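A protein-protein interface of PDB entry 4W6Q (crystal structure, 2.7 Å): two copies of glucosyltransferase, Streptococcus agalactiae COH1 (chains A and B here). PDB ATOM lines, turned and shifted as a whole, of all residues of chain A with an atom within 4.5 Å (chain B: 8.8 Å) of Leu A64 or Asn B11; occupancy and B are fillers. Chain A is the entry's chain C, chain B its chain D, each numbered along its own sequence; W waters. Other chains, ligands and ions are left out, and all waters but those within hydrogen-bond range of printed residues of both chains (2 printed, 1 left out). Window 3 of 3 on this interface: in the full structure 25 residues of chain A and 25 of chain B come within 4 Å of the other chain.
Of chain B, only Asn B11 comes within 4 Å of Leu A64. Of chain A, only Ser A62, Gly A63, Leu A64 and Arg A65 come within 4 Å of Asn B11. Of the printed residues of chain A, Gln B20 touches Arg A65. Printed residues of chain A within 4 Å of Gly B39: Ser A62 (2.9 Å). Printed residues of chain B within 4 Å of Gly A63: Asn B11 (3.2 Å) and Glu B37 (3.99 Å). Of the printed residues of chain B, Ser A62 touches Asn B11 (2.5 Å), Gly B39 (2.9 Å), Ile B40 (3.4 Å) and His B41 (3.5 Å). Printed residues of chain A within 4 Å of Glu B37: Tyr A6 and Gly A63. Ile B21 touches none of the printed residues of chain A. The nearest printed residue of chain B that does not touch Leu A64 is His B41 (5.6 Å). The nearest printed residue of chain A that does not touch Asn B11 is Arg A4 (4.8 Å).
Hydrophobic or aromatic side chains of chain B within 4 Å of the printed part of chain A: His B41. Hydrophobic or aromatic side chains of chain A within 4 Å of the printed part of chain B: Tyr A6.
NH2 of Arg A4 is in hydrogen-bond range of O of Gly A63, 2.7 Å away. The backbone carbonyl oxygen of Asn B11 is in hydrogen-bond range of the backbone NH of Ser B42. The side-chain hydroxyl (OH) of Tyr A6 lies within hydrogen-bond range of the backbone carbonyl oxygen (O) of Gly A63 (3.1 Å). The side-chain amide nitrogen of Asn B24 is in hydrogen-bond range of the backbone carbonyl oxygen of Gln B20. The side-chain carboxylate (OD2) of Asp A68 lies within hydrogen-bond range of the backbone NH (N) of Arg A65 (3.1 Å). OE1 of Gln B20 lies within hydrogen-bond range of N of His B13 (2.9 Å).
Water W1 bridges O of Gly B39 (2.7 Å) and OG of Ser A62 (3.1 Å). Water W2 lies within hydrogen-bond range of the guanidinium group (NH2) of Arg A65 (3.1 Å), the side-chain amide oxygen (OD1) of Asn B11 (3.2 Å) and the backbone carbonyl oxygen (O) of Leu B10 (3.4 Å).
OG of Ser A62 sits at hydrogen-bond distance from O of Gly B39 (2.9 Å). OD1 of Asn B11 is in hydrogen-bond range of NE of Arg A65 (3.1 Å). NH2 of Arg A65 lies close to NE2 of Gln B20, at 2.8 Å. NH2 of Arg A65 is in hydrogen-bond range of OD1 of Asn B24. The side-chain hydroxyl of Tyr A6 lies within hydrogen-bond range of the side-chain carboxylate of Glu B37 (2.7 Å). The backbone NH of Ile B40 lies within hydrogen-bond range of the side-chain hydroxyl of Ser A62, 3.4 Å away. The backbone carbonyl oxygen of Ser A62 is in hydrogen-bond range of the side-chain amide nitrogen of Asn B11 (2.5 Å). ND2 of Asn B11 sits close to O of Gly A63, at 3.3 Å. ND2 of Asn B11 sits at hydrogen-bond distance from O of Leu A64.
Position printed for both chains: 38. Of the 11 pairs that touch across the chains among the printed residues, none has its exchanged pair printed and touching as well.
Among the printed residues, merely in contact across the chains: Ser A62 with His B41 (3.5 Å) and Gly A63 with Glu B37 (3.99 Å).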
ATOM      1  N   ARG A   4      15.533 -21.283  -0.643  1.00  0.00           N
ATOM      2  CA  ARG A   4      16.074 -20.336  -1.617  1.00  0.00           C
ATOM      3  C   ARG A   4      16.766 -19.225  -0.807  1.00  0.00           C
ATOM      4  O   ARG A   4      16.405 -18.992   0.341  1.00  0.00           O
ATOM      5  CB  ARG A   4      14.958 -19.824  -2.554  1.00  0.00           C
ATOM      6  CG  ARG A   4      13.985 -20.953  -2.987  1.00  0.00           C
ATOM      7  CD  ARG A   4      12.596 -20.494  -3.447  1.00  0.00           C
ATOM      8  NE  ARG A   4      11.850 -19.970  -2.310  1.00  0.00           N
ATOM      9  CZ  ARG A   4      11.017 -18.944  -2.395  1.00  0.00           C
ATOM     10  NH1 ARG A   4      10.800 -18.366  -3.567  1.00  0.00           N
ATOM     11  NH2 ARG A   4      10.415 -18.482  -1.313  1.00  0.00           N
ATOM     12  N   TYR A   6      17.858 -15.219  -0.427  1.00  0.00           N
ATOM     13  CA  TYR A   6      17.555 -13.869  -0.891  1.00  0.00           C
ATOM     14  C   TYR A   6      18.537 -12.829  -0.358  1.00  0.00           C
ATOM     15  O   TYR A   6      19.057 -12.952   0.755  1.00  0.00           O
ATOM     16  CB  TYR A   6      16.133 -13.475  -0.492  1.00  0.00           C
ATOM     17  CG  TYR A   6      15.055 -14.108  -1.334  1.00  0.00           C
ATOM     18  CD1 TYR A   6      14.566 -15.371  -1.036  1.00  0.00           C
ATOM     19  CD2 TYR A   6      14.518 -13.435  -2.417  1.00  0.00           C
ATOM     20  CE1 TYR A   6      13.565 -15.957  -1.805  1.00  0.00           C
ATOM     21  CE2 TYR A   6      13.520 -13.993  -3.187  1.00  0.00           C
ATOM     22  CZ  TYR A   6      13.047 -15.264  -2.881  1.00  0.00           C
ATOM     23  OH  TYR A   6      12.057 -15.838  -3.650  1.00  0.00           O
ATOM     24  N   LEU A  38      16.091  -9.098  -3.493  1.00  0.00           N
ATOM     25  CA  LEU A  38      14.964  -8.358  -2.899  1.00  0.00           C
ATOM     26  C   LEU A  38      15.180  -6.883  -3.163  1.00  0.00           C
ATOM     27  O   LEU A  38      15.822  -6.198  -2.373  1.00  0.00           O
ATOM     28  CB  LEU A  38      14.834  -8.605  -1.397  1.00  0.00           C
ATOM     29  CG  LEU A  38      14.411 -10.034  -1.093  1.00  0.00           C
ATOM     30  CD1 LEU A  38      14.246 -10.277   0.395  1.00  0.00           C
ATOM     31  CD2 LEU A  38      13.120 -10.318  -1.838  1.00  0.00           C
ATOM     32  N   CYS A  61       8.717  -8.338  -0.268  1.00  0.00           N
ATOM     33  CA  CYS A  61       8.997  -9.617   0.363  1.00  0.00           C
ATOM     34  C   CYS A  61       8.091 -10.756  -0.056  1.00  0.00           C
ATOM     35  O   CYS A  61       8.219 -11.872   0.461  1.00  0.00           O
ATOM     36  CB  CYS A  61       8.905  -9.471   1.878  1.00  0.00           C
ATOM     37  SG  CYS A  61      10.233  -8.509   2.570  1.00  0.00           S
ATOM     38  N   SER A  62       7.177 -10.485  -0.977  1.00  0.00           N
ATOM     39  CA  SER A  62       6.151 -11.471  -1.299  1.00  0.00           C
ATOM     40  C   SER A  62       6.742 -12.839  -1.676  1.00  0.00           C
ATOM     41  O   SER A  62       6.200 -13.876  -1.294  1.00  0.00           O
ATOM     42  CB  SER A  62       5.250 -10.945  -2.418  1.00  0.00           C
ATOM     43  OG  SER A  62       6.010 -10.513  -3.524  1.00  0.00           O
ATOM     44  N   GLY A  63       7.873 -12.833  -2.380  1.00  0.00           N
ATOM     45  CA  GLY A  63       8.515 -14.061  -2.815  1.00  0.00           C
ATOM     46  C   GLY A  63       9.056 -14.975  -1.726  1.00  0.00           C
ATOM     47  O   GLY A  63       9.428 -16.110  -2.002  1.00  0.00           O
ATOM     48  N   LEU A  64       9.101 -14.503  -0.488  1.00  0.00           N
ATOM     49  CA  LEU A  64       9.678 -15.304   0.580  1.00  0.00           C
ATOM     50  C   LEU A  64       8.780 -16.471   0.981  1.00  0.00           C
ATOM     51  O   LEU A  64       7.561 -16.399   0.907  1.00  0.00           O
ATOM     52  CB  LEU A  64       9.979 -14.436   1.802  1.00  0.00           C
ATOM     53  CG  LEU A  64      10.973 -13.301   1.536  1.00  0.00           C
ATOM     54  CD1 LEU A  64      11.314 -12.498   2.796  1.00  0.00           C
ATOM     55  CD2 LEU A  64      12.239 -13.862   0.900  1.00  0.00           C
ATOM     56  N   ARG A  65       9.410 -17.561   1.386  1.00  0.00           N
ATOM     57  CA  ARG A  65       8.699 -18.671   1.979  1.00  0.00           C
ATOM     58  C   ARG A  65       9.420 -19.041   3.247  1.00  0.00           C
ATOM     59  O   ARG A  65      10.571 -18.679   3.426  1.00  0.00           O
ATOM     60  CB  ARG A  65       8.632 -19.860   1.028  1.00  0.00           C
ATOM     61  CG  ARG A  65       7.775 -19.610  -0.193  1.00  0.00           C
ATOM     62  CD  ARG A  65       7.964 -20.723  -1.189  1.00  0.00           C
ATOM     63  NE  ARG A  65       7.077 -20.624  -2.345  1.00  0.00           N
ATOM     64  CZ  ARG A  65       7.215 -21.362  -3.444  1.00  0.00           C
ATOM     65  NH1 ARG A  65       8.221 -22.231  -3.546  1.00  0.00           N
ATOM     66  NH2 ARG A  65       6.362 -21.221  -4.449  1.00  0.00           N
ATOM     67  N   ASP A  68      13.480 -20.189   3.897  1.00  0.00           N
ATOM     68  CA  ASP A  68      14.447 -19.542   3.028  1.00  0.00           C
ATOM     69  C   ASP A  68      15.539 -18.910   3.872  1.00  0.00           C
ATOM     70  O   ASP A  68      15.510 -19.010   5.099  1.00  0.00           O
ATOM     71  CB  ASP A  68      13.795 -18.468   2.176  1.00  0.00           C
ATOM     72  CG  ASP A  68      12.920 -19.034   1.105  1.00  0.00           C
ATOM     73  OD1 ASP A  68      12.914 -20.272   0.941  1.00  0.00           O
ATOM     74  OD2 ASP A  68      12.243 -18.235   0.419  1.00  0.00           O
ATOM     75  N   VAL A  70      17.487 -14.992   4.059  1.00  0.00           N
ATOM     76  CA  VAL A  70      17.573 -13.622   3.573  1.00  0.00           C
ATOM     77  C   VAL A  70      18.826 -12.950   4.108  1.00  0.00           C
ATOM     78  O   VAL A  70      19.126 -13.004   5.311  1.00  0.00           O
ATOM     79  CB  VAL A  70      16.332 -12.796   3.959  1.00  0.00           C
ATOM     80  CG1 VAL A  70      16.515 -11.310   3.607  1.00  0.00           C
ATOM     81  CG2 VAL A  70      15.116 -13.352   3.260  1.00  0.00           C
ATOM     82  N   LEU A  90      10.829  -9.645   8.237  1.00  0.00           N
ATOM     83  CA  LEU A  90      11.596 -10.846   8.010  1.00  0.00           C
ATOM     84  C   LEU A  90      11.414 -11.821   9.162  1.00  0.00           C
ATOM     85  O   LEU A  90      11.570 -13.026   8.998  1.00  0.00           O
ATOM     86  CB  LEU A  90      13.075 -10.512   7.823  1.00  0.00           C
ATOM     87  CG  LEU A  90      13.387  -9.558   6.674  1.00  0.00           C
ATOM     88  CD1 LEU A  90      14.821  -9.092   6.752  1.00  0.00           C
ATOM     89  CD2 LEU A  90      13.113 -10.182   5.334  1.00  0.00           C
ATOM     90  N   PHE A  93       8.547 -14.410   9.284  1.00  0.00           N
ATOM     91  CA  PHE A  93       8.774 -15.569   8.428  1.00  0.00           C
ATOM     92  C   PHE A  93       9.647 -16.583   9.177  1.00  0.00           C
ATOM     93  O   PHE A  93      10.472 -16.200   9.999  1.00  0.00           O
ATOM     94  CB  PHE A  93       9.438 -15.166   7.123  1.00  0.00           C
ATOM     95  CG  PHE A  93       8.523 -14.522   6.109  1.00  0.00           C
ATOM     96  CD1 PHE A  93       8.377 -13.150   6.052  1.00  0.00           C
ATOM     97  CD2 PHE A  93       7.882 -15.285   5.148  1.00  0.00           C
ATOM     98  CE1 PHE A  93       7.570 -12.557   5.078  1.00  0.00           C
ATOM     99  CE2 PHE A  93       7.070 -14.690   4.176  1.00  0.00           C
ATOM    100  CZ  PHE A  93       6.914 -13.328   4.142  1.00  0.00           C
ATOM    101  N   THR B   8       8.053 -12.104 -13.472  1.00  0.00           N
ATOM    102  CA  THR B   8       7.077 -12.130 -12.379  1.00  0.00           C
ATOM    103  C   THR B   8       6.799 -13.565 -11.958  1.00  0.00           C
ATOM    104  O   THR B   8       6.802 -14.472 -12.788  1.00  0.00           O
ATOM    105  CB  THR B   8       5.743 -11.419 -12.758  1.00  0.00           C
ATOM    106  OG1 THR B   8       5.184 -11.991 -13.950  1.00  0.00           O
ATOM    107  CG2 THR B   8       5.989  -9.950 -12.993  1.00  0.00           C
ATOM    108  N   ASN B   9       6.564 -13.762 -10.661  1.00  0.00           N
ATOM    109  CA  ASN B   9       6.377 -15.099 -10.109  1.00  0.00           C
ATOM    110  C   ASN B   9       5.408 -15.141  -8.903  1.00  0.00           C
ATOM    111  O   ASN B   9       5.642 -14.486  -7.886  1.00  0.00           O
ATOM    112  CB  ASN B   9       7.744 -15.684  -9.721  1.00  0.00           C
ATOM    113  CG  ASN B   9       7.672 -17.162  -9.333  1.00  0.00           C
ATOM    114  OD1 ASN B   9       6.876 -17.926  -9.873  1.00  0.00           O
ATOM    115  ND2 ASN B   9       8.518 -17.567  -8.402  1.00  0.00           N
ATOM    116  N   LEU B  10       4.341 -15.937  -9.028  1.00  0.00           N
ATOM    117  CA  LEU B  10       3.351 -16.158  -7.955  1.00  0.00           C
ATOM    118  C   LEU B  10       3.865 -16.797  -6.683  1.00  0.00           C
ATOM    119  O   LEU B  10       4.751 -17.660  -6.708  1.00  0.00           O
ATOM    120  CB  LEU B  10       2.226 -17.054  -8.433  1.00  0.00           C
ATOM    121  CG  LEU B  10       1.456 -16.519  -9.609  1.00  0.00           C
ATOM    122  CD1 LEU B  10       0.260 -17.399  -9.784  1.00  0.00           C
ATOM    123  CD2 LEU B  10       1.112 -15.042  -9.388  1.00  0.00           C
ATOM    124  N   ASN B  11       3.239 -16.413  -5.575  1.00  0.00           N
ATOM    125  CA  ASN B  11       3.522 -16.998  -4.272  1.00  0.00           C
ATOM    126  C   ASN B  11       2.251 -16.993  -3.409  1.00  0.00           C
ATOM    127  O   ASN B  11       1.418 -16.078  -3.524  1.00  0.00           O
ATOM    128  CB  ASN B  11       4.658 -16.234  -3.589  1.00  0.00           C
ATOM    129  CG  ASN B  11       5.290 -17.010  -2.461  1.00  0.00           C
ATOM    130  OD1 ASN B  11       5.061 -18.205  -2.314  1.00  0.00           O
ATOM    131  ND2 ASN B  11       6.115 -16.342  -1.672  1.00  0.00           N
ATOM    132  N   GLY B  12       2.085 -18.023  -2.580  1.00  0.00           N
ATOM    133  CA  GLY B  12       0.987 -18.066  -1.627  1.00  0.00           C
ATOM    134  C   GLY B  12      -0.263 -18.857  -2.007  1.00  0.00           C
ATOM    135  O   GLY B  12      -1.265 -18.819  -1.285  1.00  0.00           O
ATOM    136  N   HIS B  13      -0.224 -19.571  -3.130  1.00  0.00           N
ATOM    137  CA  HIS B  13      -1.268 -20.553  -3.430  1.00  0.00           C
ATOM    138  C   HIS B  13      -1.016 -21.862  -2.700  1.00  0.00           C
ATOM    139  O   HIS B  13       0.059 -22.079  -2.131  1.00  0.00           O
ATOM    140  CB  HIS B  13      -1.355 -20.840  -4.916  1.00  0.00           C
ATOM    141  CG  HIS B  13      -1.961 -19.738  -5.715  1.00  0.00           C
ATOM    142  ND1 HIS B  13      -2.466 -19.932  -6.983  1.00  0.00           N
ATOM    143  CD2 HIS B  13      -2.140 -18.427  -5.435  1.00  0.00           C
ATOM    144  CE1 HIS B  13      -2.932 -18.787  -7.450  1.00  0.00           C
ATOM    145  NE2 HIS B  13      -2.746 -17.857  -6.530  1.00  0.00           N
ATOM    146  N   SER B  14      -2.009 -22.744  -2.745  1.00  0.00           N
ATOM    147  CA  SER B  14      -1.916 -24.047  -2.100  1.00  0.00           C
ATOM    148  C   SER B  14      -0.787 -24.904  -2.646  1.00  0.00           C
ATOM    149  O   SER B  14      -0.308 -24.691  -3.761  1.00  0.00           O
ATOM    150  CB  SER B  14      -3.226 -24.810  -2.256  1.00  0.00           C
ATOM    151  OG  SER B  14      -3.020 -26.195  -2.023  1.00  0.00           O
ATOM    152  N   SER B  17      -1.588 -26.254  -6.195  1.00  0.00           N
ATOM    153  CA  SER B  17      -1.898 -25.318  -7.275  1.00  0.00           C
ATOM    154  C   SER B  17      -0.938 -25.420  -8.476  1.00  0.00           C
ATOM    155  O   SER B  17       0.246 -25.101  -8.370  1.00  0.00           O
ATOM    156  CB  SER B  17      -1.894 -23.890  -6.740  1.00  0.00           C
ATOM    157  OG  SER B  17      -1.984 -22.972  -7.816  1.00  0.00           O
ATOM    158  N   ALA B  19      -1.162 -23.764 -11.337  1.00  0.00           N
ATOM    159  CA  ALA B  19      -0.880 -22.433 -11.860  1.00  0.00           C
ATOM    160  C   ALA B  19       0.390 -21.856 -11.254  1.00  0.00           C
ATOM    161  O   ALA B  19       1.256 -21.378 -11.984  1.00  0.00           O
ATOM    162  CB  ALA B  19      -2.046 -21.498 -11.612  1.00  0.00           C
ATOM    163  N   GLN B  20       0.506 -21.920  -9.928  1.00  0.00           N
ATOM    164  CA  GLN B  20       1.692 -21.419  -9.236  1.00  0.00           C
ATOM    165  C   GLN B  20       2.932 -22.213  -9.593  1.00  0.00           C
ATOM    166  O   GLN B  20       3.960 -21.643  -9.950  1.00  0.00           O
ATOM    167  CB  GLN B  20       1.507 -21.440  -7.717  1.00  0.00           C
ATOM    168  CG  GLN B  20       2.814 -21.364  -6.920  1.00  0.00           C
ATOM    169  CD  GLN B  20       2.642 -20.735  -5.537  1.00  0.00           C
ATOM    170  OE1 GLN B  20       1.717 -19.954  -5.304  1.00  0.00           O
ATOM    171  NE2 GLN B  20       3.542 -21.066  -4.620  1.00  0.00           N
ATOM    172  N   ILE B  21       2.849 -23.532  -9.507  1.00  0.00           N
ATOM    173  CA  ILE B  21       4.060 -24.318  -9.684  1.00  0.00           C
ATOM    174  C   ILE B  21       4.554 -24.356 -11.134  1.00  0.00           C
ATOM    175  O   ILE B  21       5.749 -24.480 -11.350  1.00  0.00           O
ATOM    176  CB  ILE B  21       3.873 -25.737  -9.155  1.00  0.00           C
ATOM    177  CG1 ILE B  21       3.155 -26.618 -10.176  1.00  0.00           C
ATOM    178  CG2 ILE B  21       3.156 -25.685  -7.798  1.00  0.00           C
ATOM    179  CD1 ILE B  21       3.266 -28.085  -9.862  1.00  0.00           C
ATOM    180  N   GLN B  23       4.463 -21.711 -12.902  1.00  0.00           N
ATOM    181  CA  GLN B  23       5.168 -20.428 -12.839  1.00  0.00           C
ATOM    182  C   GLN B  23       6.452 -20.485 -12.016  1.00  0.00           C
ATOM    183  O   GLN B  23       7.428 -19.817 -12.334  1.00  0.00           O
ATOM    184  CB  GLN B  23       4.254 -19.357 -12.256  1.00  0.00           C
ATOM    185  CG  GLN B  23       3.676 -18.396 -13.283  1.00  0.00           C
ATOM    186  CD  GLN B  23       2.911 -17.256 -12.638  1.00  0.00           C
ATOM    187  OE1 GLN B  23       3.457 -16.511 -11.824  1.00  0.00           O
ATOM    188  NE2 GLN B  23       1.640 -17.122 -12.992  1.00  0.00           N
ATOM    189  N   ASN B  24       6.448 -21.262 -10.941  1.00  0.00           N
ATOM    190  CA  ASN B  24       7.640 -21.392 -10.110  1.00  0.00           C
ATOM    191  C   ASN B  24       8.763 -22.064 -10.855  1.00  0.00           C
ATOM    192  O   ASN B  24       9.923 -21.689 -10.727  1.00  0.00           O
ATOM    193  CB  ASN B  24       7.341 -22.181  -8.839  1.00  0.00           C
ATOM    194  CG  ASN B  24       6.557 -21.376  -7.846  1.00  0.00           C
ATOM    195  OD1 ASN B  24       6.182 -21.868  -6.786  1.00  0.00           O
ATOM    196  ND2 ASN B  24       6.289 -20.130  -8.189  1.00  0.00           N
ATOM    197  N   THR B  27      10.339 -19.900 -13.293  1.00  0.00           N
ATOM    198  CA  THR B  27      11.161 -18.941 -12.578  1.00  0.00           C
ATOM    199  C   THR B  27      12.505 -19.545 -12.220  1.00  0.00           C
ATOM    200  O   THR B  27      13.537 -18.867 -12.262  1.00  0.00           O
ATOM    201  CB  THR B  27      10.443 -18.456 -11.312  1.00  0.00           C
ATOM    202  OG1 THR B  27       9.136 -18.003 -11.677  1.00  0.00           O
ATOM    203  CG2 THR B  27      11.211 -17.323 -10.650  1.00  0.00           C
ATOM    204  N   GLU B  37      13.813 -12.436 -10.124  1.00  0.00           N
ATOM    205  CA  GLU B  37      12.404 -12.579  -9.743  1.00  0.00           C
ATOM    206  C   GLU B  37      11.720 -11.289  -9.276  1.00  0.00           C
ATOM    207  O   GLU B  37      12.242 -10.571  -8.423  1.00  0.00           O
ATOM    208  CB  GLU B  37      12.294 -13.617  -8.632  1.00  0.00           C
ATOM    209  CG  GLU B  37      10.937 -13.785  -8.039  1.00  0.00           C
ATOM    210  CD  GLU B  37      10.956 -14.713  -6.828  1.00  0.00           C
ATOM    211  OE1 GLU B  37      10.689 -15.925  -6.992  1.00  0.00           O
ATOM    212  OE2 GLU B  37      11.251 -14.233  -5.708  1.00  0.00           O
ATOM    213  N   LEU B  38      10.551 -11.004  -9.844  1.00  0.00           N
ATOM    214  CA  LEU B  38       9.614 -10.055  -9.245  1.00  0.00           C
ATOM    215  C   LEU B  38       8.544 -10.882  -8.549  1.00  0.00           C
ATOM    216  O   LEU B  38       7.554 -11.271  -9.168  1.00  0.00           O
ATOM    217  CB  LEU B  38       8.992  -9.124 -10.287  1.00  0.00           C
ATOM    218  CG  LEU B  38       9.968  -8.227 -11.046  1.00  0.00           C
ATOM    219  CD1 LEU B  38       9.271  -7.469 -12.169  1.00  0.00           C
ATOM    220  CD2 LEU B  38      10.681  -7.252 -10.108  1.00  0.00           C
ATOM    221  N   GLY B  39       8.765 -11.192  -7.277  1.00  0.00           N
ATOM    222  CA  GLY B  39       7.812 -11.988  -6.522  1.00  0.00           C
ATOM    223  C   GLY B  39       6.447 -11.332  -6.414  1.00  0.00           C
ATOM    224  O   GLY B  39       6.353 -10.110  -6.331  1.00  0.00           O
ATOM    225  N   ILE B  40       5.387 -12.135  -6.435  1.00  0.00           N
ATOM    226  CA  ILE B  40       4.016 -11.625  -6.331  1.00  0.00           C
ATOM    227  C   ILE B  40       3.185 -12.561  -5.491  1.00  0.00           C
ATOM    228  O   ILE B  40       3.070 -13.737  -5.839  1.00  0.00           O
ATOM    229  CB  ILE B  40       3.355 -11.478  -7.710  1.00  0.00           C
ATOM    230  CG1 ILE B  40       4.125 -10.452  -8.542  1.00  0.00           C
ATOM    231  CG2 ILE B  40       1.900 -11.041  -7.571  1.00  0.00           C
ATOM    232  CD1 ILE B  40       3.721 -10.400  -9.980  1.00  0.00           C
ATOM    233  N   HIS B  41       2.617 -12.047  -4.393  1.00  0.00           N
ATOM    234  CA  HIS B  41       1.763 -12.842  -3.488  1.00  0.00           C
ATOM    235  C   HIS B  41       0.293 -12.727  -3.864  1.00  0.00           C
ATOM    236  O   HIS B  41      -0.177 -11.667  -4.280  1.00  0.00           O
ATOM    237  CB  HIS B  41       1.966 -12.411  -2.027  1.00  0.00           C
ATOM    238  CG  HIS B  41       1.660 -13.483  -1.016  1.00  0.00           C
ATOM    239  ND1 HIS B  41       0.400 -13.676  -0.488  1.00  0.00           N
ATOM    240  CD2 HIS B  41       2.461 -14.399  -0.417  1.00  0.00           C
ATOM    241  CE1 HIS B  41       0.436 -14.671   0.384  1.00  0.00           C
ATOM    242  NE2 HIS B  41       1.675 -15.124   0.451  1.00  0.00           N
ATOM    243  N   SER B  42      -0.436 -13.827  -3.718  1.00  0.00           N
ATOM    244  CA  SER B  42      -1.845 -13.837  -4.085  1.00  0.00           C
ATOM    245  C   SER B  42      -2.711 -13.609  -2.836  1.00  0.00           C
ATOM    246  O   SER B  42      -2.516 -14.284  -1.823  1.00  0.00           O
ATOM    247  CB  SER B  42      -2.199 -15.151  -4.774  1.00  0.00           C
ATOM    248  OG  SER B  42      -1.353 -15.387  -5.896  1.00  0.00           O
ATOM    249  N   TYR B  43      -3.641 -12.655  -2.933  1.00  0.00           N
ATOM    250  CA  TYR B  43      -4.449 -12.195  -1.823  1.00  0.00           C
ATOM    251  C   TYR B  43      -5.709 -11.477  -2.363  1.00  0.00           C
ATOM    252  O   TYR B  43      -5.686 -11.026  -3.512  1.00  0.00           O
ATOM    253  CB  TYR B  43      -3.637 -11.257  -0.912  1.00  0.00           C
ATOM    254  CG  TYR B  43      -3.292  -9.935  -1.566  1.00  0.00           C
ATOM    255  CD1 TYR B  43      -4.080  -8.822  -1.361  1.00  0.00           C
ATOM    256  CD2 TYR B  43      -2.198  -9.806  -2.403  1.00  0.00           C
ATOM    257  CE1 TYR B  43      -3.792  -7.609  -1.946  1.00  0.00           C
ATOM    258  CE2 TYR B  43      -1.901  -8.591  -3.000  1.00  0.00           C
ATOM    259  CZ  TYR B  43      -2.716  -7.497  -2.762  1.00  0.00           C
ATOM    260  OH  TYR B  43      -2.473  -6.272  -3.321  1.00  0.00           O
ATOM    261  N   THR B  76      -1.881 -13.366 -12.847  1.00  0.00           N
ATOM    262  CA  THR B  76      -1.430 -13.330 -11.455  1.00  0.00           C
ATOM    263  C   THR B  76      -2.365 -14.023 -10.465  1.00  0.00           C
ATOM    264  O   THR B  76      -1.942 -14.369  -9.363  1.00  0.00           O
ATOM    265  CB  THR B  76      -1.268 -11.885 -10.957  1.00  0.00           C
ATOM    266  OG1 THR B  76      -2.538 -11.213 -11.020  1.00  0.00           O
ATOM    267  CG2 THR B  76      -0.230 -11.127 -11.786  1.00  0.00           C
ATOM    268  N   TRP B  77      -3.633 -14.188 -10.845  1.00  0.00           N
ATOM    269  CA  TRP B  77      -4.675 -14.678  -9.936  1.00  0.00           C
ATOM    270  C   TRP B  77      -4.869 -13.751  -8.753  1.00  0.00           C
ATOM    271  O   TRP B  77      -5.195 -14.189  -7.653  1.00  0.00           O
ATOM    272  CB  TRP B  77      -4.353 -16.088  -9.440  1.00  0.00           C
ATOM    273  CG  TRP B  77      -4.238 -17.023 -10.557  1.00  0.00           C
ATOM    274  CD1 TRP B  77      -3.096 -17.541 -11.082  1.00  0.00           C
ATOM    275  CD2 TRP B  77      -5.311 -17.517 -11.350  1.00  0.00           C
ATOM    276  NE1 TRP B  77      -3.394 -18.353 -12.149  1.00  0.00           N
ATOM    277  CE2 TRP B  77      -4.753 -18.355 -12.332  1.00  0.00           C
ATOM    278  CE3 TRP B  77      -6.695 -17.334 -11.323  1.00  0.00           C
ATOM    279  CZ2 TRP B  77      -5.529 -19.017 -13.273  1.00  0.00           C
ATOM    280  CZ3 TRP B  77      -7.465 -17.991 -12.256  1.00  0.00           C
ATOM    281  CH2 TRP B  77      -6.882 -18.824 -13.221  1.00  0.00           C
ATOM    282  N   ASN B  78      -4.644 -12.466  -8.984  1.00  0.00           N
ATOM    283  CA  ASN B  78      -4.908 -11.463  -7.978  1.00  0.00           C
ATOM    284  C   ASN B  78      -6.058 -10.614  -8.453  1.00  0.00           C
ATOM    285  O   ASN B  78      -6.488  -9.673  -7.776  1.00  0.00           O
ATOM    286  CB  ASN B  78      -3.666 -10.644  -7.705  1.00  0.00           C
ATOM    287  CG  ASN B  78      -2.976 -11.109  -6.476  1.00  0.00           C
ATOM    288  OD1 ASN B  78      -3.404 -12.094  -5.888  1.00  0.00           O
ATOM    289  ND2 ASN B  78      -1.921 -10.419  -6.062  1.00  0.00           N
HETATM  290  O   HOH W   1       8.357  -9.053  -4.835  1.00  0.00           O
HETATM  291  O   HOH W   2       7.372 -18.261  -4.581  1.00  0.00           O
